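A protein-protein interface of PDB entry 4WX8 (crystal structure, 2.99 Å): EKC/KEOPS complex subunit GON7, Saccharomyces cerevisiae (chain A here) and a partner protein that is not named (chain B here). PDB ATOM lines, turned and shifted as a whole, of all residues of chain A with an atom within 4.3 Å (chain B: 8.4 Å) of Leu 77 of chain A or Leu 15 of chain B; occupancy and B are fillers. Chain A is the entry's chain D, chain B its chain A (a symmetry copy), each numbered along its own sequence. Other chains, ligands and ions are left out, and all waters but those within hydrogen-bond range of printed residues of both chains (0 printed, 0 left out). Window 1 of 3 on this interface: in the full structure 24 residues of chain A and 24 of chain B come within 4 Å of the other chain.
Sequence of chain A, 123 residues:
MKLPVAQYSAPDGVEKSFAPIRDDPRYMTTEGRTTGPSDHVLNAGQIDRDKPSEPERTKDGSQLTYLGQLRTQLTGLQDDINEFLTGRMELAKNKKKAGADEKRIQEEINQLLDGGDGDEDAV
N of Lys 16 of chain B is in hydrogen-bond range of O of Val 5 of chain A, 3.0 Å away. The backbone carbonyl oxygen (O) of Ser 71 of chain B lies within hydrogen-bond range of the side-chain amide nitrogen (NE2) of Gln 78 of chain A. The side-chain amide nitrogen of Gln 78 of chain A sits at hydrogen-bond distance from the side-chain carboxylate of Asp 75 of chain B, 2.8 Å away. The side-chain amino group of Lys 78 of chain B lies within hydrogen-bond range of the side-chain amide oxygen of Gln 78 of chain A (2.8 Å).
The backbone NH of Leu 15 of chain B lies within hydrogen-bond range of the backbone carbonyl oxygen of Val 56 of chain B (2.8 Å). The side-chain carboxylate of Asp 75 of chain B lies within salt-bridge range of the side-chain amino group of Lys 78 of chain B (3.7 Å). O of Ala 6 of chain A sits at hydrogen-bond distance from N of Phe 18 of chain A, at 2.8 Å.
Leu 15 of chain B touches Val 5 of chain A. Ala 6 of chain A touches Glu 14 of chain B. CD1 of Leu 74 of chain A touches CG2 of Ile 77 of chain B (3.8 Å). Lys 78 of chain B touches Leu 74 of chain A (CG to CD1, 3.97 Å). Thr 75 of chain A touches Lys 78 of chain B. CD1 of Leu 15 of chain B touches CD2 of Leu 77 of chain A (3.2 Å). Ile 74 of chain B touches Gln 78 of chain A (CB to NE2, 3.9 Å).
Of the printed residues of chain B, Val 5 of chain A touches Leu 15 and Lys 16. No residue of chain B comes within 4 Å of Gly 76 of chain A. Printed residues of chain B within 4 Å of Gln 78 of chain A: Ser 71 (3.1 Å), Ile 74 (3.9 Å), Asp 75 (2.8 Å) and Lys 78 (2.8 Å). Of chain A, only Val 5 and Leu 77 come within 4 Å of Leu 15 of chain B. Printed residues of chain A within 4 Å of Ser 71 of chain B: Gln 78 (3.1 Å). Of the printed residues of chain A, Asp 75 of chain B touches Gln 78 (2.8 Å). Of the printed residues of chain A, Ile 77 of chain B touches Leu 74 (3.8 Å). The nearest residue of chain B that does not touch Leu 77 of chain A is Ile 74 of chain B (5.2 Å). The nearest printed residue of chain A that does not touch Leu 15 of chain B is Ala 6 of chain A (4.3 Å).
Hydrophobic or aromatic side chains of chain B that line the printed part of chain A: Leu 15, Ile 74 and Ile 77. Of the 13 printed residues of chain A, 6 touch a printed residue of chain B. Hydrophobic or aromatic side chains of chain A that line the printed part of chain B: Val 5, Ala 6, Leu 74 and Leu 77. Among the printed residues, 11 pairs touch across the chains.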
ATOM      1  N   VAL A   5     -14.523   3.153  23.246  1.00  0.00           N
ATOM      2  CA  VAL A   5     -13.387   2.505  23.882  1.00  0.00           C
ATOM      3  C   VAL A   5     -12.605   1.747  22.822  1.00  0.00           C
ATOM      4  O   VAL A   5     -13.143   1.462  21.728  1.00  0.00           O
ATOM      5  CB  VAL A   5     -13.844   1.482  24.939  1.00  0.00           C
ATOM      6  CG1 VAL A   5     -14.488   2.189  26.125  1.00  0.00           C
ATOM      7  CG2 VAL A   5     -14.772   0.441  24.310  1.00  0.00           C
ATOM      8  N   ALA A   6     -11.355   1.407  23.152  1.00  0.00           N
ATOM      9  CA  ALA A   6     -10.568   0.566  22.274  1.00  0.00           C
ATOM     10  C   ALA A   6      -9.779  -0.418  23.117  1.00  0.00           C
ATOM     11  O   ALA A   6      -9.499  -0.121  24.263  1.00  0.00           O
ATOM     12  CB  ALA A   6      -9.642   1.426  21.432  1.00  0.00           C
ATOM     13  N   PHE A  18      -8.006   1.520  26.026  1.00  0.00           N
ATOM     14  CA  PHE A  18      -8.189   2.952  25.959  1.00  0.00           C
ATOM     15  C   PHE A  18      -9.573   3.337  26.428  1.00  0.00           C
ATOM     16  O   PHE A  18     -10.531   2.572  26.269  1.00  0.00           O
ATOM     17  CB  PHE A  18      -8.048   3.406  24.520  1.00  0.00           C
ATOM     18  CG  PHE A  18      -6.760   3.006  23.890  1.00  0.00           C
ATOM     19  CD1 PHE A  18      -6.611   1.764  23.348  1.00  0.00           C
ATOM     20  CD2 PHE A  18      -5.687   3.896  23.843  1.00  0.00           C
ATOM     21  CE1 PHE A  18      -5.424   1.403  22.760  1.00  0.00           C
ATOM     22  CE2 PHE A  18      -4.509   3.552  23.242  1.00  0.00           C
ATOM     23  CZ  PHE A  18      -4.372   2.295  22.704  1.00  0.00           C
ATOM     24  N   ALA A  19      -9.685   4.547  26.957  1.00  0.00           N
ATOM     25  CA  ALA A  19     -10.959   5.078  27.373  1.00  0.00           C
ATOM     26  C   ALA A  19     -10.760   6.515  27.713  1.00  0.00           C
ATOM     27  O   ALA A  19      -9.951   6.825  28.578  1.00  0.00           O
ATOM     28  CB  ALA A  19     -11.455   4.344  28.594  1.00  0.00           C
ATOM     29  N   GLN A  73     -14.781  12.686  21.904  1.00  0.00           N
ATOM     30  CA  GLN A  73     -14.252  11.479  22.519  1.00  0.00           C
ATOM     31  C   GLN A  73     -13.512  10.606  21.518  1.00  0.00           C
ATOM     32  O   GLN A  73     -12.586   9.898  21.880  1.00  0.00           O
ATOM     33  CB  GLN A  73     -15.373  10.659  23.138  1.00  0.00           C
ATOM     34  CG  GLN A  73     -16.205  11.452  24.116  1.00  0.00           C
ATOM     35  CD  GLN A  73     -17.220  10.615  24.833  1.00  0.00           C
ATOM     36  OE1 GLN A  73     -17.853   9.744  24.238  1.00  0.00           O
ATOM     37  NE2 GLN A  73     -17.397  10.878  26.116  1.00  0.00           N
ATOM     38  N   LEU A  74     -13.925  10.648  20.258  1.00  0.00           N
ATOM     39  CA  LEU A  74     -13.287   9.821  19.255  1.00  0.00           C
ATOM     40  C   LEU A  74     -11.985  10.399  18.818  1.00  0.00           C
ATOM     41  O   LEU A  74     -11.109   9.653  18.494  1.00  0.00           O
ATOM     42  CB  LEU A  74     -14.172   9.661  18.033  1.00  0.00           C
ATOM     43  CG  LEU A  74     -15.255   8.595  18.115  1.00  0.00           C
ATOM     44  CD1 LEU A  74     -15.872   8.403  16.742  1.00  0.00           C
ATOM     45  CD2 LEU A  74     -14.698   7.274  18.602  1.00  0.00           C
ATOM     46  N   THR A  75     -11.862  11.719  18.765  1.00  0.00           N
ATOM     47  CA  THR A  75     -10.551  12.325  18.509  1.00  0.00           C
ATOM     48  C   THR A  75      -9.667  12.106  19.720  1.00  0.00           C
ATOM     49  O   THR A  75      -8.454  12.019  19.599  1.00  0.00           O
ATOM     50  CB  THR A  75     -10.592  13.848  18.302  1.00  0.00           C
ATOM     51  OG1 THR A  75     -11.165  14.465  19.461  1.00  0.00           O
ATOM     52  CG2 THR A  75     -11.367  14.226  17.053  1.00  0.00           C
ATOM     53  N   GLY A  76     -10.286  12.043  20.889  1.00  0.00           N
ATOM     54  CA  GLY A  76      -9.560  11.697  22.077  1.00  0.00           C
ATOM     55  C   GLY A  76      -8.916  10.336  21.919  1.00  0.00           C
ATOM     56  O   GLY A  76      -7.726  10.154  22.140  1.00  0.00           O
ATOM     57  N   LEU A  77      -9.715   9.374  21.521  1.00  0.00           N
ATOM     58  CA  LEU A  77      -9.262   8.016  21.368  1.00  0.00           C
ATOM     59  C   LEU A  77      -8.300   7.900  20.198  1.00  0.00           C
ATOM     60  O   LEU A  77      -7.314   7.184  20.261  1.00  0.00           O
ATOM     61  CB  LEU A  77     -10.479   7.133  21.112  1.00  0.00           C
ATOM     62  CG  LEU A  77     -10.367   5.657  21.454  1.00  0.00           C
ATOM     63  CD1 LEU A  77     -10.224   5.474  22.957  1.00  0.00           C
ATOM     64  CD2 LEU A  77     -11.590   4.922  20.926  1.00  0.00           C
ATOM     65  N   GLN A  78      -8.607   8.594  19.117  1.00  0.00           N
ATOM     66  CA  GLN A  78      -7.786   8.523  17.915  1.00  0.00           C
ATOM     67  C   GLN A  78      -6.376   8.957  18.250  1.00  0.00           C
ATOM     68  O   GLN A  78      -5.392   8.356  17.810  1.00  0.00           O
ATOM     69  CB  GLN A  78      -8.323   9.470  16.855  1.00  0.00           C
ATOM     70  CG  GLN A  78      -7.634   9.325  15.519  1.00  0.00           C
ATOM     71  CD  GLN A  78      -8.226  10.241  14.484  1.00  0.00           C
ATOM     72  OE1 GLN A  78      -8.690  11.318  14.813  1.00  0.00           O
ATOM     73  NE2 GLN A  78      -8.215   9.816  13.228  1.00  0.00           N
ATOM     74  N   ASP A  79      -6.304  10.045  19.013  1.00  0.00           N
ATOM     75  CA  ASP A  79      -5.065  10.558  19.567  1.00  0.00           C
ATOM     76  C   ASP A  79      -4.369   9.496  20.420  1.00  0.00           C
ATOM     77  O   ASP A  79      -3.326   8.941  20.026  1.00  0.00           O
ATOM     78  CB  ASP A  79      -5.375  11.802  20.389  1.00  0.00           C
ATOM     79  CG  ASP A  79      -5.555  13.048  19.521  1.00  0.00           C
ATOM     80  OD1 ASP A  79      -5.347  12.956  18.293  1.00  0.00           O
ATOM     81  OD2 ASP A  79      -5.880  14.135  20.053  1.00  0.00           O
ATOM     82  N   ASP A  80      -4.963   9.210  21.577  1.00  0.00           N
ATOM     83  CA  ASP A  80      -4.519   8.115  22.434  1.00  0.00           C
ATOM     84  C   ASP A  80      -3.822   7.030  21.634  1.00  0.00           C
ATOM     85  O   ASP A  80      -2.643   6.733  21.832  1.00  0.00           O
ATOM     86  CB  ASP A  80      -5.718   7.480  23.134  1.00  0.00           C
ATOM     87  CG  ASP A  80      -6.120   8.217  24.384  1.00  0.00           C
ATOM     88  OD1 ASP A  80      -5.744   9.418  24.489  1.00  0.00           O
ATOM     89  OD2 ASP A  80      -6.798   7.584  25.257  1.00  0.00           O
ATOM     90  N   ILE A  81      -4.583   6.442  20.726  1.00  0.00           N
ATOM     91  CA  ILE A  81      -4.110   5.335  19.921  1.00  0.00           C
ATOM     92  C   ILE A  81      -2.911   5.766  19.096  1.00  0.00           C
ATOM     93  O   ILE A  81      -1.965   5.018  18.965  1.00  0.00           O
ATOM     94  CB  ILE A  81      -5.248   4.781  19.019  1.00  0.00           C
ATOM     95  CG1 ILE A  81      -6.311   4.110  19.893  1.00  0.00           C
ATOM     96  CG2 ILE A  81      -4.712   3.793  17.995  1.00  0.00           C
ATOM     97  CD1 ILE A  81      -7.622   3.874  19.195  1.00  0.00           C
ATOM     98  N   THR B  12      -3.401  -6.357  17.163  1.00  0.00           N
ATOM     99  CA  THR B  12      -4.844  -6.358  17.137  1.00  0.00           C
ATOM    100  C   THR B  12      -5.397  -5.181  17.886  1.00  0.00           C
ATOM    101  O   THR B  12      -4.913  -4.858  18.963  1.00  0.00           O
ATOM    102  CB  THR B  12      -5.337  -7.614  17.858  1.00  0.00           C
ATOM    103  OG1 THR B  12      -5.238  -8.720  16.954  1.00  0.00           O
ATOM    104  CG2 THR B  12      -6.775  -7.433  18.355  1.00  0.00           C
ATOM    105  N   LEU B  13      -6.435  -4.564  17.338  1.00  0.00           N
ATOM    106  CA  LEU B  13      -7.133  -3.516  18.041  1.00  0.00           C
ATOM    107  C   LEU B  13      -8.618  -3.527  17.702  1.00  0.00           C
ATOM    108  O   LEU B  13      -8.992  -3.439  16.537  1.00  0.00           O
ATOM    109  CB  LEU B  13      -6.533  -2.186  17.671  1.00  0.00           C
ATOM    110  CG  LEU B  13      -7.148  -1.041  18.450  1.00  0.00           C
ATOM    111  CD1 LEU B  13      -6.086   0.004  18.825  1.00  0.00           C
ATOM    112  CD2 LEU B  13      -8.257  -0.436  17.592  1.00  0.00           C
ATOM    113  N   GLU B  14      -9.457  -3.627  18.727  1.00  0.00           N
ATOM    114  CA  GLU B  14     -10.881  -3.475  18.545  1.00  0.00           C
ATOM    115  C   GLU B  14     -11.332  -2.129  19.096  1.00  0.00           C
ATOM    116  O   GLU B  14     -10.882  -1.677  20.141  1.00  0.00           O
ATOM    117  CB  GLU B  14     -11.639  -4.607  19.261  1.00  0.00           C
ATOM    118  CG  GLU B  14     -12.924  -5.064  18.568  1.00  0.00           C
ATOM    119  CD  GLU B  14     -14.003  -5.568  19.533  1.00  0.00           C
ATOM    120  OE1 GLU B  14     -14.127  -4.952  20.611  1.00  0.00           O
ATOM    121  OE2 GLU B  14     -14.742  -6.559  19.230  1.00  0.00           O
ATOM    122  N   LEU B  15     -12.266  -1.526  18.379  1.00  0.00           N
ATOM    123  CA  LEU B  15     -12.833  -0.231  18.691  1.00  0.00           C
ATOM    124  C   LEU B  15     -14.362  -0.431  18.781  1.00  0.00           C
ATOM    125  O   LEU B  15     -14.992  -0.814  17.794  1.00  0.00           O
ATOM    126  CB  LEU B  15     -12.450   0.702  17.548  1.00  0.00           C
ATOM    127  CG  LEU B  15     -12.985   2.137  17.447  1.00  0.00           C
ATOM    128  CD1 LEU B  15     -12.555   2.974  18.636  1.00  0.00           C
ATOM    129  CD2 LEU B  15     -12.518   2.817  16.160  1.00  0.00           C
ATOM    130  N   LYS B  16     -14.938  -0.229  19.973  1.00  0.00           N
ATOM    131  CA  LYS B  16     -16.380  -0.364  20.227  1.00  0.00           C
ATOM    132  C   LYS B  16     -17.021   1.024  20.387  1.00  0.00           C
ATOM    133  O   LYS B  16     -16.724   1.728  21.352  1.00  0.00           O
ATOM    134  CB  LYS B  16     -16.622  -1.115  21.542  1.00  0.00           C
ATOM    135  CG  LYS B  16     -15.620  -2.214  21.898  1.00  0.00           C
ATOM    136  N   ILE B  17     -17.920   1.407  19.488  1.00  0.00           N
ATOM    137  CA  ILE B  17     -18.479   2.758  19.487  1.00  0.00           C
ATOM    138  C   ILE B  17     -19.994   2.786  19.737  1.00  0.00           C
ATOM    139  O   ILE B  17     -20.766   2.228  18.945  1.00  0.00           O
ATOM    140  CB  ILE B  17     -18.289   3.357  18.107  1.00  0.00           C
ATOM    141  CG1 ILE B  17     -16.812   3.398  17.758  1.00  0.00           C
ATOM    142  CG2 ILE B  17     -18.904   4.735  18.009  1.00  0.00           C
ATOM    143  CD1 ILE B  17     -16.574   3.163  16.278  1.00  0.00           C
ATOM    144  N   PRO B  18     -20.440   3.449  20.824  1.00  0.00           N
ATOM    145  CA  PRO B  18     -21.858   3.520  21.170  1.00  0.00           C
ATOM    146  C   PRO B  18     -22.671   4.675  20.570  1.00  0.00           C
ATOM    147  O   PRO B  18     -22.411   5.833  20.850  1.00  0.00           O
ATOM    148  CB  PRO B  18     -21.845   3.665  22.685  1.00  0.00           C
ATOM    149  CG  PRO B  18     -20.442   3.880  23.108  1.00  0.00           C
ATOM    150  CD  PRO B  18     -19.597   4.015  21.886  1.00  0.00           C
ATOM    151  N   LEU B  32     -20.407   2.958   6.369  1.00  0.00           N
ATOM    152  CA  LEU B  32     -18.962   2.912   6.485  1.00  0.00           C
ATOM    153  C   LEU B  32     -18.125   2.429   5.309  1.00  0.00           C
ATOM    154  O   LEU B  32     -17.091   3.020   5.044  1.00  0.00           O
ATOM    155  CB  LEU B  32     -18.539   2.099   7.684  1.00  0.00           C
ATOM    156  CG  LEU B  32     -17.055   2.269   8.047  1.00  0.00           C
ATOM    157  CD1 LEU B  32     -16.781   3.699   8.397  1.00  0.00           C
ATOM    158  CD2 LEU B  32     -16.690   1.432   9.242  1.00  0.00           C
ATOM    159  N   VAL B  45      -9.592  -5.225   8.343  1.00  0.00           N
ATOM    160  CA  VAL B  45     -10.606  -4.685   9.243  1.00  0.00           C
ATOM    161  C   VAL B  45     -11.996  -5.367   9.106  1.00  0.00           C
ATOM    162  O   VAL B  45     -12.471  -5.696   7.990  1.00  0.00           O
ATOM    163  CB  VAL B  45     -10.724  -3.176   9.011  1.00  0.00           C
ATOM    164  CG1 VAL B  45     -11.001  -2.897   7.563  1.00  0.00           C
ATOM    165  CG2 VAL B  45     -11.779  -2.586   9.914  1.00  0.00           C
ATOM    166  N   ASP B  46     -12.627  -5.591  10.259  1.00  0.00           N
ATOM    167  CA  ASP B  46     -13.986  -6.120  10.318  1.00  0.00           C
ATOM    168  C   ASP B  46     -14.904  -5.161  11.055  1.00  0.00           C
ATOM    169  O   ASP B  46     -14.652  -4.824  12.217  1.00  0.00           O
ATOM    170  CB  ASP B  46     -13.972  -7.473  11.006  1.00  0.00           C
ATOM    171  CG  ASP B  46     -13.203  -8.501  10.204  1.00  0.00           C
ATOM    172  OD1 ASP B  46     -12.747  -8.085   9.110  1.00  0.00           O
ATOM    173  OD2 ASP B  46     -13.038  -9.681  10.643  1.00  0.00           O
ATOM    174  N   TYR B  47     -15.949  -4.685  10.377  1.00  0.00           N
ATOM    175  CA  TYR B  47     -16.979  -3.898  11.079  1.00  0.00           C
ATOM    176  C   TYR B  47     -18.298  -4.625  11.283  1.00  0.00           C
ATOM    177  O   TYR B  47     -18.622  -5.568  10.600  1.00  0.00           O
ATOM    178  CB  TYR B  47     -17.236  -2.552  10.417  1.00  0.00           C
ATOM    179  CG  TYR B  47     -17.402  -2.604   8.955  1.00  0.00           C
ATOM    180  CD1 TYR B  47     -16.329  -2.808   8.131  1.00  0.00           C
ATOM    181  CD2 TYR B  47     -18.613  -2.405   8.388  1.00  0.00           C
ATOM    182  CE1 TYR B  47     -16.476  -2.845   6.763  1.00  0.00           C
ATOM    183  CE2 TYR B  47     -18.783  -2.441   7.012  1.00  0.00           C
ATOM    184  CZ  TYR B  47     -17.712  -2.669   6.212  1.00  0.00           C
ATOM    185  OH  TYR B  47     -17.859  -2.718   4.853  1.00  0.00           O
ATOM    186  N   SER B  48     -19.059  -4.187  12.262  1.00  0.00           N
ATOM    187  CA  SER B  48     -20.375  -4.740  12.477  1.00  0.00           C
ATOM    188  C   SER B  48     -21.014  -4.007  13.624  1.00  0.00           C
ATOM    189  O   SER B  48     -20.409  -3.140  14.238  1.00  0.00           O
ATOM    190  CB  SER B  48     -20.314  -6.246  12.762  1.00  0.00           C
ATOM    191  OG  SER B  48     -19.736  -6.495  14.004  1.00  0.00           O
ATOM    192  N   VAL B  53     -24.147  -0.642  19.594  1.00  0.00           N
ATOM    193  CA  VAL B  53     -22.697  -0.481  19.555  1.00  0.00           C
ATOM    194  C   VAL B  53     -22.197  -0.900  18.195  1.00  0.00           C
ATOM    195  O   VAL B  53     -22.705  -1.867  17.619  1.00  0.00           O
ATOM    196  CB  VAL B  53     -21.968  -1.390  20.555  1.00  0.00           C
ATOM    197  CG1 VAL B  53     -20.457  -1.218  20.413  1.00  0.00           C
ATOM    198  CG2 VAL B  53     -22.444  -1.120  21.975  1.00  0.00           C
ATOM    199  N   MET B  54     -21.194  -0.185  17.691  1.00  0.00           N
ATOM    200  CA  MET B  54     -20.549  -0.567  16.425  1.00  0.00           C
ATOM    201  C   MET B  54     -19.242  -1.219  16.772  1.00  0.00           C
ATOM    202  O   MET B  54     -18.454  -0.676  17.555  1.00  0.00           O
ATOM    203  CB  MET B  54     -20.283   0.634  15.513  1.00  0.00           C
ATOM    204  CG  MET B  54     -19.556   0.217  14.232  1.00  0.00           C
ATOM    205  SD  MET B  54     -19.134   1.762  13.056  1.00  0.00           S
ATOM    206  CE  MET B  54     -20.645   2.943  13.379  1.00  0.00           C
ATOM    207  N   LEU B  55     -18.998  -2.392  16.208  1.00  0.00           N
ATOM    208  CA  LEU B  55     -17.778  -3.069  16.460  1.00  0.00           C
ATOM    209  C   LEU B  55     -16.853  -2.964  15.258  1.00  0.00           C
ATOM    210  O   LEU B  55     -17.201  -3.428  14.177  1.00  0.00           O
ATOM    211  CB  LEU B  55     -18.087  -4.518  16.752  1.00  0.00           C
ATOM    212  CG  LEU B  55     -19.009  -4.625  17.968  1.00  0.00           C
ATOM    213  CD1 LEU B  55     -19.130  -6.075  18.394  1.00  0.00           C
ATOM    214  CD2 LEU B  55     -18.523  -3.796  19.144  1.00  0.00           C
ATOM    215  N   VAL B  56     -15.668  -2.365  15.438  1.00  0.00           N
ATOM    216  CA  VAL B  56     -14.662  -2.396  14.397  1.00  0.00           C
ATOM    217  C   VAL B  56     -13.436  -3.122  14.897  1.00  0.00           C
ATOM    218  O   VAL B  56     -12.831  -2.714  15.890  1.00  0.00           O
ATOM    219  CB  VAL B  56     -14.211  -0.998  13.993  1.00  0.00           C
ATOM    220  CG1 VAL B  56     -13.448  -1.076  12.676  1.00  0.00           C
ATOM    221  CG2 VAL B  56     -15.390  -0.052  13.869  1.00  0.00           C
ATOM    222  N   GLN B  57     -13.045  -4.168  14.177  1.00  0.00           N
ATOM    223  CA  GLN B  57     -11.917  -5.008  14.564  1.00  0.00           C
ATOM    224  C   GLN B  57     -10.804  -4.965  13.526  1.00  0.00           C
ATOM    225  O   GLN B  57     -10.982  -5.364  12.360  1.00  0.00           O
ATOM    226  CB  GLN B  57     -12.357  -6.429  14.690  1.00  0.00           C
ATOM    227  CG  GLN B  57     -11.216  -7.349  14.998  1.00  0.00           C
ATOM    228  CD  GLN B  57     -10.939  -7.398  16.478  1.00  0.00           C
ATOM    229  OE1 GLN B  57     -11.794  -7.843  17.262  1.00  0.00           O
ATOM    230  NE2 GLN B  57      -9.735  -6.937  16.884  1.00  0.00           N
ATOM    231  N   PHE B  58      -9.645  -4.485  13.974  1.00  0.00           N
ATOM    232  CA  PHE B  58      -8.493  -4.362  13.133  1.00  0.00           C
ATOM    233  C   PHE B  58      -7.566  -5.507  13.421  1.00  0.00           C
ATOM    234  O   PHE B  58      -7.533  -5.988  14.559  1.00  0.00           O
ATOM    235  CB  PHE B  58      -7.812  -3.082  13.464  1.00  0.00           C
ATOM    236  CG  PHE B  58      -8.667  -1.879  13.276  1.00  0.00           C
ATOM    237  CD1 PHE B  58      -9.497  -1.447  14.281  1.00  0.00           C
ATOM    238  CD2 PHE B  58      -8.613  -1.159  12.102  1.00  0.00           C
ATOM    239  CE1 PHE B  58     -10.263  -0.306  14.121  1.00  0.00           C
ATOM    240  CE2 PHE B  58      -9.391  -0.026  11.924  1.00  0.00           C
ATOM    241  CZ  PHE B  58     -10.218   0.403  12.929  1.00  0.00           C
ATOM    242  N   VAL B  70      -5.884   2.410  11.230  1.00  0.00           N
ATOM    243  CA  VAL B  70      -6.879   2.741  12.234  1.00  0.00           C
ATOM    244  C   VAL B  70      -7.238   4.213  12.215  1.00  0.00           C
ATOM    245  O   VAL B  70      -8.406   4.551  12.310  1.00  0.00           O
ATOM    246  CB  VAL B  70      -6.420   2.374  13.648  1.00  0.00           C
ATOM    247  CG1 VAL B  70      -7.342   2.998  14.689  1.00  0.00           C
ATOM    248  CG2 VAL B  70      -6.417   0.860  13.816  1.00  0.00           C
ATOM    249  N   SER B  71      -6.264   5.106  12.101  1.00  0.00           N
ATOM    250  CA  SER B  71      -6.619   6.508  12.157  1.00  0.00           C
ATOM    251  C   SER B  71      -7.617   6.797  11.022  1.00  0.00           C
ATOM    252  O   SER B  71      -8.654   7.452  11.255  1.00  0.00           O
ATOM    253  CB  SER B  71      -5.394   7.429  12.087  1.00  0.00           C
ATOM    254  N   ILE B  73      -9.672   5.055   9.400  1.00  0.00           N
ATOM    255  CA  ILE B  73     -11.000   4.550   9.621  1.00  0.00           C
ATOM    256  C   ILE B  73     -11.710   5.461  10.614  1.00  0.00           C
ATOM    257  O   ILE B  73     -12.729   6.093  10.303  1.00  0.00           O
ATOM    258  CB  ILE B  73     -10.947   3.106  10.132  1.00  0.00           C
ATOM    259  CG1 ILE B  73     -10.562   2.168   8.977  1.00  0.00           C
ATOM    260  CG2 ILE B  73     -12.284   2.713  10.742  1.00  0.00           C
ATOM    261  CD1 ILE B  73     -11.575   2.107   7.848  1.00  0.00           C
ATOM    262  N   ILE B  74     -11.165   5.559  11.807  1.00  0.00           N
ATOM    263  CA  ILE B  74     -11.733   6.492  12.745  1.00  0.00           C
ATOM    264  C   ILE B  74     -12.217   7.769  12.019  1.00  0.00           C
ATOM    265  O   ILE B  74     -13.248   8.345  12.361  1.00  0.00           O
ATOM    266  CB  ILE B  74     -10.691   6.887  13.787  1.00  0.00           C
ATOM    267  CG1 ILE B  74     -10.087   5.635  14.447  1.00  0.00           C
ATOM    268  CG2 ILE B  74     -11.335   7.819  14.804  1.00  0.00           C
ATOM    269  CD1 ILE B  74     -10.468   5.428  15.895  1.00  0.00           C
ATOM    270  N   ASP B  75     -11.470   8.221  11.016  1.00  0.00           N
ATOM    271  CA  ASP B  75     -11.819   9.469  10.352  1.00  0.00           C
ATOM    272  C   ASP B  75     -13.168   9.340   9.644  1.00  0.00           C
ATOM    273  O   ASP B  75     -14.021  10.243   9.680  1.00  0.00           O
ATOM    274  CB  ASP B  75     -10.727   9.861   9.345  1.00  0.00           C
ATOM    275  CG  ASP B  75      -9.656  10.778   9.949  1.00  0.00           C
ATOM    276  OD1 ASP B  75      -9.730  11.045  11.167  1.00  0.00           O
ATOM    277  OD2 ASP B  75      -8.753  11.242   9.200  1.00  0.00           O
ATOM    278  N   ILE B  77     -15.499   7.191  10.356  1.00  0.00           N
ATOM    279  CA  ILE B  77     -16.500   7.067  11.390  1.00  0.00           C
ATOM    280  C   ILE B  77     -16.981   8.416  11.878  1.00  0.00           C
ATOM    281  O   ILE B  77     -18.182   8.660  11.960  1.00  0.00           O
ATOM    282  CB  ILE B  77     -15.946   6.275  12.574  1.00  0.00           C
ATOM    283  CG1 ILE B  77     -15.612   4.857  12.093  1.00  0.00           C
ATOM    284  CG2 ILE B  77     -16.927   6.310  13.724  1.00  0.00           C
ATOM    285  CD1 ILE B  77     -15.009   3.954  13.131  1.00  0.00           C
ATOM    286  N   LYS B  78     -16.036   9.286  12.208  1.00  0.00           N
ATOM    287  CA  LYS B  78     -16.358  10.615  12.700  1.00  0.00           C
ATOM    288  C   LYS B  78     -17.256  11.324  11.708  1.00  0.00           C
ATOM    289  O   LYS B  78     -18.211  12.022  12.080  1.00  0.00           O
ATOM    290  CB  LYS B  78     -15.076  11.410  12.900  1.00  0.00           C
ATOM    291  CG  LYS B  78     -14.414  11.134  14.249  1.00  0.00           C
ATOM    292  CD  LYS B  78     -12.901  11.284  14.212  1.00  0.00           C
ATOM    293  CE  LYS B  78     -12.479  12.727  14.314  1.00  0.00           C
ATOM    294  NZ  LYS B  78     -11.000  12.770  14.202  1.00  0.00           N
